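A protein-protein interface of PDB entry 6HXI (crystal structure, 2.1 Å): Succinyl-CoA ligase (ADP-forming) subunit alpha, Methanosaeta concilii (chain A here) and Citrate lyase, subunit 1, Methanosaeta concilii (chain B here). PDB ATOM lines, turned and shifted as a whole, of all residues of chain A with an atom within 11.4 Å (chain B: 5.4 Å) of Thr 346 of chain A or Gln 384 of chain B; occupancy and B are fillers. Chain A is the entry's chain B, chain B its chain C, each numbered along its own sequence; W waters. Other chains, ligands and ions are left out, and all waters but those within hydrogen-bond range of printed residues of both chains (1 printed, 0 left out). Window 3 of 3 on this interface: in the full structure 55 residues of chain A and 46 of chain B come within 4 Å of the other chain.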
ATOM      1  N   ARG A  27       1.233 -39.707   0.094  1.00  0.00           N
ATOM      2  CA  ARG A  27       1.632 -39.497   1.491  1.00  0.00           C
ATOM      3  C   ARG A  27       3.121 -39.752   1.662  1.00  0.00           C
ATOM      4  O   ARG A  27       3.809 -38.943   2.292  1.00  0.00           O
ATOM      5  CB  ARG A  27       0.812 -40.387   2.445  1.00  0.00           C
ATOM      6  CG  ARG A  27      -0.624 -39.920   2.575  1.00  0.00           C
ATOM      7  CD  ARG A  27      -1.272 -40.406   3.826  1.00  0.00           C
ATOM      8  NE  ARG A  27      -2.508 -39.672   4.069  1.00  0.00           N
ATOM      9  CZ  ARG A  27      -3.715 -40.160   3.835  1.00  0.00           C
ATOM     10  NH1 ARG A  27      -4.789 -39.431   4.087  1.00  0.00           N
ATOM     11  NH2 ARG A  27      -3.860 -41.380   3.334  1.00  0.00           N
ATOM     12  N   THR A 157      -1.776 -37.319   7.874  1.00  0.00           N
ATOM     13  CA  THR A 157      -1.651 -36.073   7.100  1.00  0.00           C
ATOM     14  C   THR A 157      -0.335 -35.358   7.311  1.00  0.00           C
ATOM     15  O   THR A 157       0.286 -35.519   8.364  1.00  0.00           O
ATOM     16  CB  THR A 157      -2.849 -35.138   7.378  1.00  0.00           C
ATOM     17  OG1 THR A 157      -2.795 -34.659   8.725  1.00  0.00           O
ATOM     18  CG2 THR A 157      -4.200 -35.824   7.131  1.00  0.00           C
ATOM     19  N   GLU A 159      -0.070 -32.253   7.943  1.00  0.00           N
ATOM     20  CA  GLU A 159      -0.345 -31.379   9.098  1.00  0.00           C
ATOM     21  C   GLU A 159       0.028 -32.110  10.395  1.00  0.00           C
ATOM     22  O   GLU A 159       0.725 -31.556  11.244  1.00  0.00           O
ATOM     23  CB  GLU A 159      -1.824 -30.932   9.114  1.00  0.00           C
ATOM     24  CG  GLU A 159      -2.077 -29.709   8.237  1.00  0.00           C
ATOM     25  CD  GLU A 159      -3.480 -29.508   7.686  1.00  0.00           C
ATOM     26  OE1 GLU A 159      -3.828 -28.344   7.382  1.00  0.00           O
ATOM     27  OE2 GLU A 159      -4.217 -30.508   7.521  1.00  0.00           O
ATOM     28  N   THR A 338      -2.101 -26.786   0.319  1.00  0.00           N
ATOM     29  CA  THR A 338      -3.296 -27.606   0.518  1.00  0.00           C
ATOM     30  C   THR A 338      -3.670 -28.202  -0.827  1.00  0.00           C
ATOM     31  O   THR A 338      -3.505 -27.541  -1.844  1.00  0.00           O
ATOM     32  CB  THR A 338      -4.436 -26.726   1.053  1.00  0.00           C
ATOM     33  OG1 THR A 338      -4.019 -26.179   2.296  1.00  0.00           O
ATOM     34  CG2 THR A 338      -5.757 -27.481   1.237  1.00  0.00           C
ATOM     35  N   ASP A 339      -4.156 -29.453  -0.830  1.00  0.00           N
ATOM     36  CA  ASP A 339      -4.634 -30.094  -2.033  1.00  0.00           C
ATOM     37  C   ASP A 339      -5.908 -29.363  -2.441  1.00  0.00           C
ATOM     38  O   ASP A 339      -6.695 -28.950  -1.584  1.00  0.00           O
ATOM     39  CB  ASP A 339      -4.894 -31.584  -1.784  1.00  0.00           C
ATOM     40  CG  ASP A 339      -3.624 -32.404  -1.672  1.00  0.00           C
ATOM     41  OD1 ASP A 339      -2.714 -32.191  -2.487  1.00  0.00           O
ATOM     42  OD2 ASP A 339      -3.557 -33.288  -0.781  1.00  0.00           O
ATOM     43  N   TYR A 340      -6.060 -29.126  -3.742  1.00  0.00           N
ATOM     44  CA  TYR A 340      -7.226 -28.471  -4.335  1.00  0.00           C
ATOM     45  C   TYR A 340      -8.531 -29.097  -3.854  1.00  0.00           C
ATOM     46  O   TYR A 340      -9.420 -28.370  -3.409  1.00  0.00           O
ATOM     47  CB  TYR A 340      -7.118 -28.572  -5.878  1.00  0.00           C
ATOM     48  CG  TYR A 340      -8.428 -28.525  -6.623  1.00  0.00           C
ATOM     49  CD1 TYR A 340      -9.137 -27.333  -6.757  1.00  0.00           C
ATOM     50  CD2 TYR A 340      -8.943 -29.662  -7.240  1.00  0.00           C
ATOM     51  CE1 TYR A 340     -10.354 -27.285  -7.429  1.00  0.00           C
ATOM     52  CE2 TYR A 340     -10.145 -29.621  -7.945  1.00  0.00           C
ATOM     53  CZ  TYR A 340     -10.828 -28.420  -8.067  1.00  0.00           C
ATOM     54  OH  TYR A 340     -11.997 -28.360  -8.788  1.00  0.00           O
ATOM     55  N   SER A 341      -8.649 -30.437  -3.949  1.00  0.00           N
ATOM     56  CA  SER A 341      -9.875 -31.161  -3.571  1.00  0.00           C
ATOM     57  C   SER A 341     -10.257 -30.936  -2.099  1.00  0.00           C
ATOM     58  O   SER A 341     -11.444 -30.865  -1.804  1.00  0.00           O
ATOM     59  CB  SER A 341      -9.751 -32.652  -3.881  1.00  0.00           C
ATOM     60  OG  SER A 341      -8.684 -33.242  -3.157  1.00  0.00           O
ATOM     61  N   LYS A 342      -9.273 -30.759  -1.205  1.00  0.00           N
ATOM     62  CA  LYS A 342      -9.546 -30.493   0.209  1.00  0.00           C
ATOM     63  C   LYS A 342     -10.114 -29.068   0.368  1.00  0.00           C
ATOM     64  O   LYS A 342     -11.164 -28.884   0.996  1.00  0.00           O
ATOM     65  CB  LYS A 342      -8.276 -30.679   1.057  1.00  0.00           C
ATOM     66  CG  LYS A 342      -8.476 -30.461   2.545  1.00  0.00           C
ATOM     67  CD  LYS A 342      -7.147 -30.456   3.281  1.00  0.00           C
ATOM     68  CE  LYS A 342      -7.267 -29.913   4.687  1.00  0.00           C
ATOM     69  NZ  LYS A 342      -5.948 -29.432   5.169  1.00  0.00           N
ATOM     70  N   ALA A 343      -9.446 -28.083  -0.260  1.00  0.00           N
ATOM     71  CA  ALA A 343      -9.845 -26.672  -0.285  1.00  0.00           C
ATOM     72  C   ALA A 343     -11.274 -26.517  -0.839  1.00  0.00           C
ATOM     73  O   ALA A 343     -12.080 -25.777  -0.277  1.00  0.00           O
ATOM     74  CB  ALA A 343      -8.865 -25.880  -1.142  1.00  0.00           C
ATOM     75  N   LEU A 344     -11.599 -27.261  -1.907  1.00  0.00           N
ATOM     76  CA  LEU A 344     -12.931 -27.203  -2.483  1.00  0.00           C
ATOM     77  C   LEU A 344     -13.985 -27.884  -1.587  1.00  0.00           C
ATOM     78  O   LEU A 344     -15.042 -27.294  -1.362  1.00  0.00           O
ATOM     79  CB  LEU A 344     -12.946 -27.762  -3.910  1.00  0.00           C
ATOM     80  CG  LEU A 344     -14.189 -27.411  -4.778  1.00  0.00           C
ATOM     81  CD1 LEU A 344     -14.349 -25.896  -4.978  1.00  0.00           C
ATOM     82  CD2 LEU A 344     -14.119 -28.084  -6.130  1.00  0.00           C
ATOM     83  N   ALA A 345     -13.687 -29.099  -1.059  1.00  0.00           N
ATOM     84  CA  ALA A 345     -14.598 -29.869  -0.195  1.00  0.00           C
ATOM     85  C   ALA A 345     -14.953 -29.146   1.103  1.00  0.00           C
ATOM     86  O   ALA A 345     -16.101 -29.214   1.547  1.00  0.00           O
ATOM     87  CB  ALA A 345     -14.024 -31.241   0.106  1.00  0.00           C
ATOM     88  N   THR A 346     -13.987 -28.416   1.675  1.00  0.00           N
ATOM     89  CA  THR A 346     -14.189 -27.664   2.907  1.00  0.00           C
ATOM     90  C   THR A 346     -14.856 -26.308   2.662  1.00  0.00           C
ATOM     91  O   THR A 346     -15.197 -25.610   3.604  1.00  0.00           O
ATOM     92  CB  THR A 346     -12.850 -27.488   3.668  1.00  0.00           C
ATOM     93  OG1 THR A 346     -11.946 -26.704   2.885  1.00  0.00           O
ATOM     94  CG2 THR A 346     -12.208 -28.813   4.076  1.00  0.00           C
ATOM     95  N   GLY A 347     -15.009 -25.919   1.414  1.00  0.00           N
ATOM     96  CA  GLY A 347     -15.562 -24.613   1.081  1.00  0.00           C
ATOM     97  C   GLY A 347     -14.576 -23.480   1.329  1.00  0.00           C
ATOM     98  O   GLY A 347     -14.975 -22.320   1.433  1.00  0.00           O
ATOM     99  N   ASP A 348     -13.273 -23.803   1.399  1.00  0.00           N
ATOM    100  CA  ASP A 348     -12.213 -22.808   1.567  1.00  0.00           C
ATOM    101  C   ASP A 348     -12.176 -21.951   0.306  1.00  0.00           C
ATOM    102  O   ASP A 348     -12.010 -20.741   0.388  1.00  0.00           O
ATOM    103  CB  ASP A 348     -10.857 -23.513   1.782  1.00  0.00           C
ATOM    104  CG  ASP A 348      -9.731 -22.625   2.311  1.00  0.00           C
ATOM    105  OD1 ASP A 348      -9.752 -22.290   3.529  1.00  0.00           O
ATOM    106  OD2 ASP A 348      -8.785 -22.337   1.537  1.00  0.00           O
ATOM    107  N   ILE A 349     -12.405 -22.587  -0.863  1.00  0.00           N
ATOM    108  CA  ILE A 349     -12.413 -21.913  -2.159  1.00  0.00           C
ATOM    109  C   ILE A 349     -13.750 -22.119  -2.865  1.00  0.00           C
ATOM    110  O   ILE A 349     -14.515 -23.028  -2.515  1.00  0.00           O
ATOM    111  CB  ILE A 349     -11.199 -22.344  -3.071  1.00  0.00           C
ATOM    112  CG1 ILE A 349     -11.274 -23.863  -3.469  1.00  0.00           C
ATOM    113  CG2 ILE A 349      -9.863 -22.008  -2.419  1.00  0.00           C
ATOM    114  CD1 ILE A 349     -10.659 -24.263  -4.807  1.00  0.00           C
ATOM    115  N   ARG A 350     -14.000 -21.307  -3.897  1.00  0.00           N
ATOM    116  CA  ARG A 350     -15.164 -21.440  -4.768  1.00  0.00           C
ATOM    117  C   ARG A 350     -14.623 -21.543  -6.174  1.00  0.00           C
ATOM    118  O   ARG A 350     -13.669 -20.848  -6.495  1.00  0.00           O
ATOM    119  CB  ARG A 350     -16.199 -20.300  -4.623  1.00  0.00           C
ATOM    120  CG  ARG A 350     -15.745 -18.922  -5.080  1.00  0.00           C
ATOM    121  CD  ARG A 350     -16.851 -17.901  -4.919  1.00  0.00           C
ATOM    122  NE  ARG A 350     -16.408 -16.612  -5.437  1.00  0.00           N
ATOM    123  CZ  ARG A 350     -17.088 -15.469  -5.382  1.00  0.00           C
ATOM    124  NH1 ARG A 350     -16.582 -14.372  -5.909  1.00  0.00           N
ATOM    125  NH2 ARG A 350     -18.281 -15.419  -4.798  1.00  0.00           N
ATOM    126  N   LYS A 351     -15.162 -22.456  -6.988  1.00  0.00           N
ATOM    127  CA  LYS A 351     -14.655 -22.623  -8.346  1.00  0.00           C
ATOM    128  C   LYS A 351     -15.791 -22.518  -9.359  1.00  0.00           C
ATOM    129  O   LYS A 351     -16.752 -23.282  -9.271  1.00  0.00           O
ATOM    130  CB  LYS A 351     -13.889 -23.954  -8.505  1.00  0.00           C
ATOM    131  CG  LYS A 351     -13.161 -24.077  -9.874  1.00  0.00           C
ATOM    132  CD  LYS A 351     -12.466 -25.411  -9.996  1.00  0.00           C
ATOM    133  CE  LYS A 351     -11.848 -25.703 -11.350  1.00  0.00           C
ATOM    134  NZ  LYS A 351     -12.838 -25.669 -12.446  1.00  0.00           N
ATOM    135  N   ALA B 349     -13.857 -37.177   7.398  1.00  0.00           N
ATOM    136  CA  ALA B 349     -14.940 -36.481   6.710  1.00  0.00           C
ATOM    137  C   ALA B 349     -15.983 -37.454   6.205  1.00  0.00           C
ATOM    138  O   ALA B 349     -17.173 -37.205   6.403  1.00  0.00           O
ATOM    139  CB  ALA B 349     -14.396 -35.662   5.554  1.00  0.00           C
ATOM    140  N   ASN B 381      -8.666 -35.237   7.035  1.00  0.00           N
ATOM    141  CA  ASN B 381      -9.806 -34.308   6.914  1.00  0.00           C
ATOM    142  C   ASN B 381     -10.609 -34.159   8.219  1.00  0.00           C
ATOM    143  O   ASN B 381     -11.803 -33.883   8.159  1.00  0.00           O
ATOM    144  CB  ASN B 381     -10.737 -34.677   5.726  1.00  0.00           C
ATOM    145  CG  ASN B 381     -10.052 -34.952   4.398  1.00  0.00           C
ATOM    146  OD1 ASN B 381     -10.148 -36.052   3.862  1.00  0.00           O
ATOM    147  ND2 ASN B 381      -9.416 -33.954   3.791  1.00  0.00           N
ATOM    148  N   TYR B 382      -9.961 -34.320   9.391  1.00  0.00           N
ATOM    149  CA  TYR B 382     -10.664 -34.245  10.677  1.00  0.00           C
ATOM    150  C   TYR B 382     -11.416 -32.941  10.865  1.00  0.00           C
ATOM    151  O   TYR B 382     -12.541 -32.996  11.346  1.00  0.00           O
ATOM    152  CB  TYR B 382      -9.757 -34.547  11.893  1.00  0.00           C
ATOM    153  CG  TYR B 382      -8.929 -33.380  12.382  1.00  0.00           C
ATOM    154  CD1 TYR B 382      -7.663 -33.138  11.866  1.00  0.00           C
ATOM    155  CD2 TYR B 382      -9.415 -32.513  13.355  1.00  0.00           C
ATOM    156  CE1 TYR B 382      -6.893 -32.066  12.316  1.00  0.00           C
ATOM    157  CE2 TYR B 382      -8.670 -31.418  13.784  1.00  0.00           C
ATOM    158  CZ  TYR B 382      -7.394 -31.216  13.284  1.00  0.00           C
ATOM    159  OH  TYR B 382      -6.617 -30.167  13.709  1.00  0.00           O
ATOM    160  N   GLU B 383     -10.810 -31.784  10.486  1.00  0.00           N
ATOM    161  CA  GLU B 383     -11.436 -30.466  10.674  1.00  0.00           C
ATOM    162  C   GLU B 383     -12.795 -30.384   9.974  1.00  0.00           C
ATOM    163  O   GLU B 383     -13.753 -29.919  10.582  1.00  0.00           O
ATOM    164  CB  GLU B 383     -10.504 -29.276  10.338  1.00  0.00           C
ATOM    165  CG  GLU B 383      -9.745 -29.278   9.017  1.00  0.00           C
ATOM    166  CD  GLU B 383      -8.434 -30.048   9.004  1.00  0.00           C
ATOM    167  OE1 GLU B 383      -8.418 -31.197   8.501  1.00  0.00           O
ATOM    168  OE2 GLU B 383      -7.440 -29.524   9.557  1.00  0.00           O
ATOM    169  N   GLN B 384     -12.900 -30.935   8.756  1.00  0.00           N
ATOM    170  CA  GLN B 384     -14.151 -31.035   7.998  1.00  0.00           C
ATOM    171  C   GLN B 384     -15.162 -31.939   8.735  1.00  0.00           C
ATOM    172  O   GLN B 384     -16.348 -31.598   8.787  1.00  0.00           O
ATOM    173  CB  GLN B 384     -13.868 -31.558   6.583  1.00  0.00           C
ATOM    174  CG  GLN B 384     -15.109 -31.716   5.706  1.00  0.00           C
ATOM    175  CD  GLN B 384     -14.825 -32.336   4.355  1.00  0.00           C
ATOM    176  OE1 GLN B 384     -13.670 -32.521   3.943  1.00  0.00           O
ATOM    177  NE2 GLN B 384     -15.887 -32.644   3.618  1.00  0.00           N
ATOM    178  N   GLY B 385     -14.689 -33.058   9.296  1.00  0.00           N
ATOM    179  CA  GLY B 385     -15.515 -33.984  10.064  1.00  0.00           C
ATOM    180  C   GLY B 385     -16.057 -33.370  11.354  1.00  0.00           C
ATOM    181  O   GLY B 385     -17.248 -33.503  11.657  1.00  0.00           O
ATOM    182  N   LEU B 386     -15.194 -32.688  12.118  1.00  0.00           N
ATOM    183  CA  LEU B 386     -15.599 -32.028  13.362  1.00  0.00           C
ATOM    184  C   LEU B 386     -16.545 -30.845  13.056  1.00  0.00           C
ATOM    185  O   LEU B 386     -17.421 -30.557  13.869  1.00  0.00           O
ATOM    186  CB  LEU B 386     -14.394 -31.544  14.203  1.00  0.00           C
ATOM    187  CG  LEU B 386     -13.290 -32.531  14.635  1.00  0.00           C
ATOM    188  CD1 LEU B 386     -12.284 -31.825  15.527  1.00  0.00           C
ATOM    189  CD2 LEU B 386     -13.836 -33.739  15.381  1.00  0.00           C
ATOM    190  N   LYS B 387     -16.383 -30.181  11.882  1.00  0.00           N
ATOM    191  CA  LYS B 387     -17.255 -29.082  11.430  1.00  0.00           C
ATOM    192  C   LYS B 387     -18.695 -29.598  11.235  1.00  0.00           C
ATOM    193  O   LYS B 387     -19.633 -28.928  11.660  1.00  0.00           O
ATOM    194  CB  LYS B 387     -16.743 -28.454  10.120  1.00  0.00           C
ATOM    195  CG  LYS B 387     -17.247 -27.025   9.885  1.00  0.00           C
ATOM    196  CD  LYS B 387     -17.326 -26.649   8.398  1.00  0.00           C
ATOM    197  CE  LYS B 387     -15.991 -26.290   7.770  1.00  0.00           C
ATOM    198  NZ  LYS B 387     -15.997 -26.503   6.297  1.00  0.00           N
ATOM    199  N   LEU B 388     -18.856 -30.790  10.607  1.00  0.00           N
ATOM    200  CA  LEU B 388     -20.139 -31.468  10.381  1.00  0.00           C
ATOM    201  C   LEU B 388     -20.847 -31.754  11.710  1.00  0.00           C
ATOM    202  O   LEU B 388     -22.048 -31.532  11.811  1.00  0.00           O
ATOM    203  CB  LEU B 388     -19.921 -32.816   9.651  1.00  0.00           C
ATOM    204  CG  LEU B 388     -19.526 -32.792   8.178  1.00  0.00           C
ATOM    205  CD1 LEU B 388     -18.976 -34.161   7.752  1.00  0.00           C
ATOM    206  CD2 LEU B 388     -20.695 -32.390   7.307  1.00  0.00           C
HETATM  207  O   HOH W   1      -6.503 -33.043   7.884  1.00  0.00           O
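O of Thr 346 of chain A lies within hydrogen-bond range of NZ of Lys 387 of chain B, 2.9 Å away.
Printed residues of chain B that touch a printed residue of chain A: Asn 381, Glu 383, Gln 384 and Lys 387.
Printed residues of chain A that touch a printed residue of chain B: Glu 159, Lys 342 and Thr 346.
Along chain A the printed residues that touch a printed residue of chain B span positions 159 to 346.
Among the printed residues, 4 pairs touch across the chains.
Among the printed residues, no Asp or Glu carboxylate lies within 4 Å of a Lys or Arg side-chain nitrogen of the other chain.
Printed residues of chain B within 4 Å of Thr 346 of chain A: Gln 384 (3.99 Å) and Lys 387 (2.9 Å).
Of the printed residues of chain A, Gln 384 of chain B touches Thr 346.
No residue of chain A comes within 4 Å of Ala 349 of chain B.
Gly 385 of chain B touches none of the printed residues of chain A.
No residue of chain A comes within 4 Å of Leu 386 of chain B.
No residue of chain A comes within 4 Å of Leu 388 of chain B.
Printed residues of chain B within 4 Å of Glu 159 of chain A: Glu 383 (3.9 Å).
Of the printed residues of chain B, Lys 342 of chain A touches Asn 381 (3.8 Å).
Water W1 lies within hydrogen-bond range of the side-chain carboxylate of Glu 383 of chain B, the backbone NH of Asn 381 of chain B and the side-chain carboxylate of Glu 159 of chain A.
OE2 of Glu 159 of chain A is in salt-bridge range of NZ of Lys 342 of chain A (3.1 Å).
OG1 of Thr 346 of chain A sits at hydrogen-bond distance from O of Ala 343 of chain A, at 3.3 Å.
The backbone carbonyl oxygen (O) of Lys 342 of chain A sits at hydrogen-bond distance from the side-chain hydroxyl (OG1) of Thr 346 of chain A (3.0 Å).
OE2 of Glu 383 of chain B touches OE2 of Glu 159 of chain A, 3.9 Å away.
CG of Lys 342 of chain A touches ND2 of Asn 381 of chain B, at 3.8 Å.
Thr 346 of chain A touches Gln 384 of chain B.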
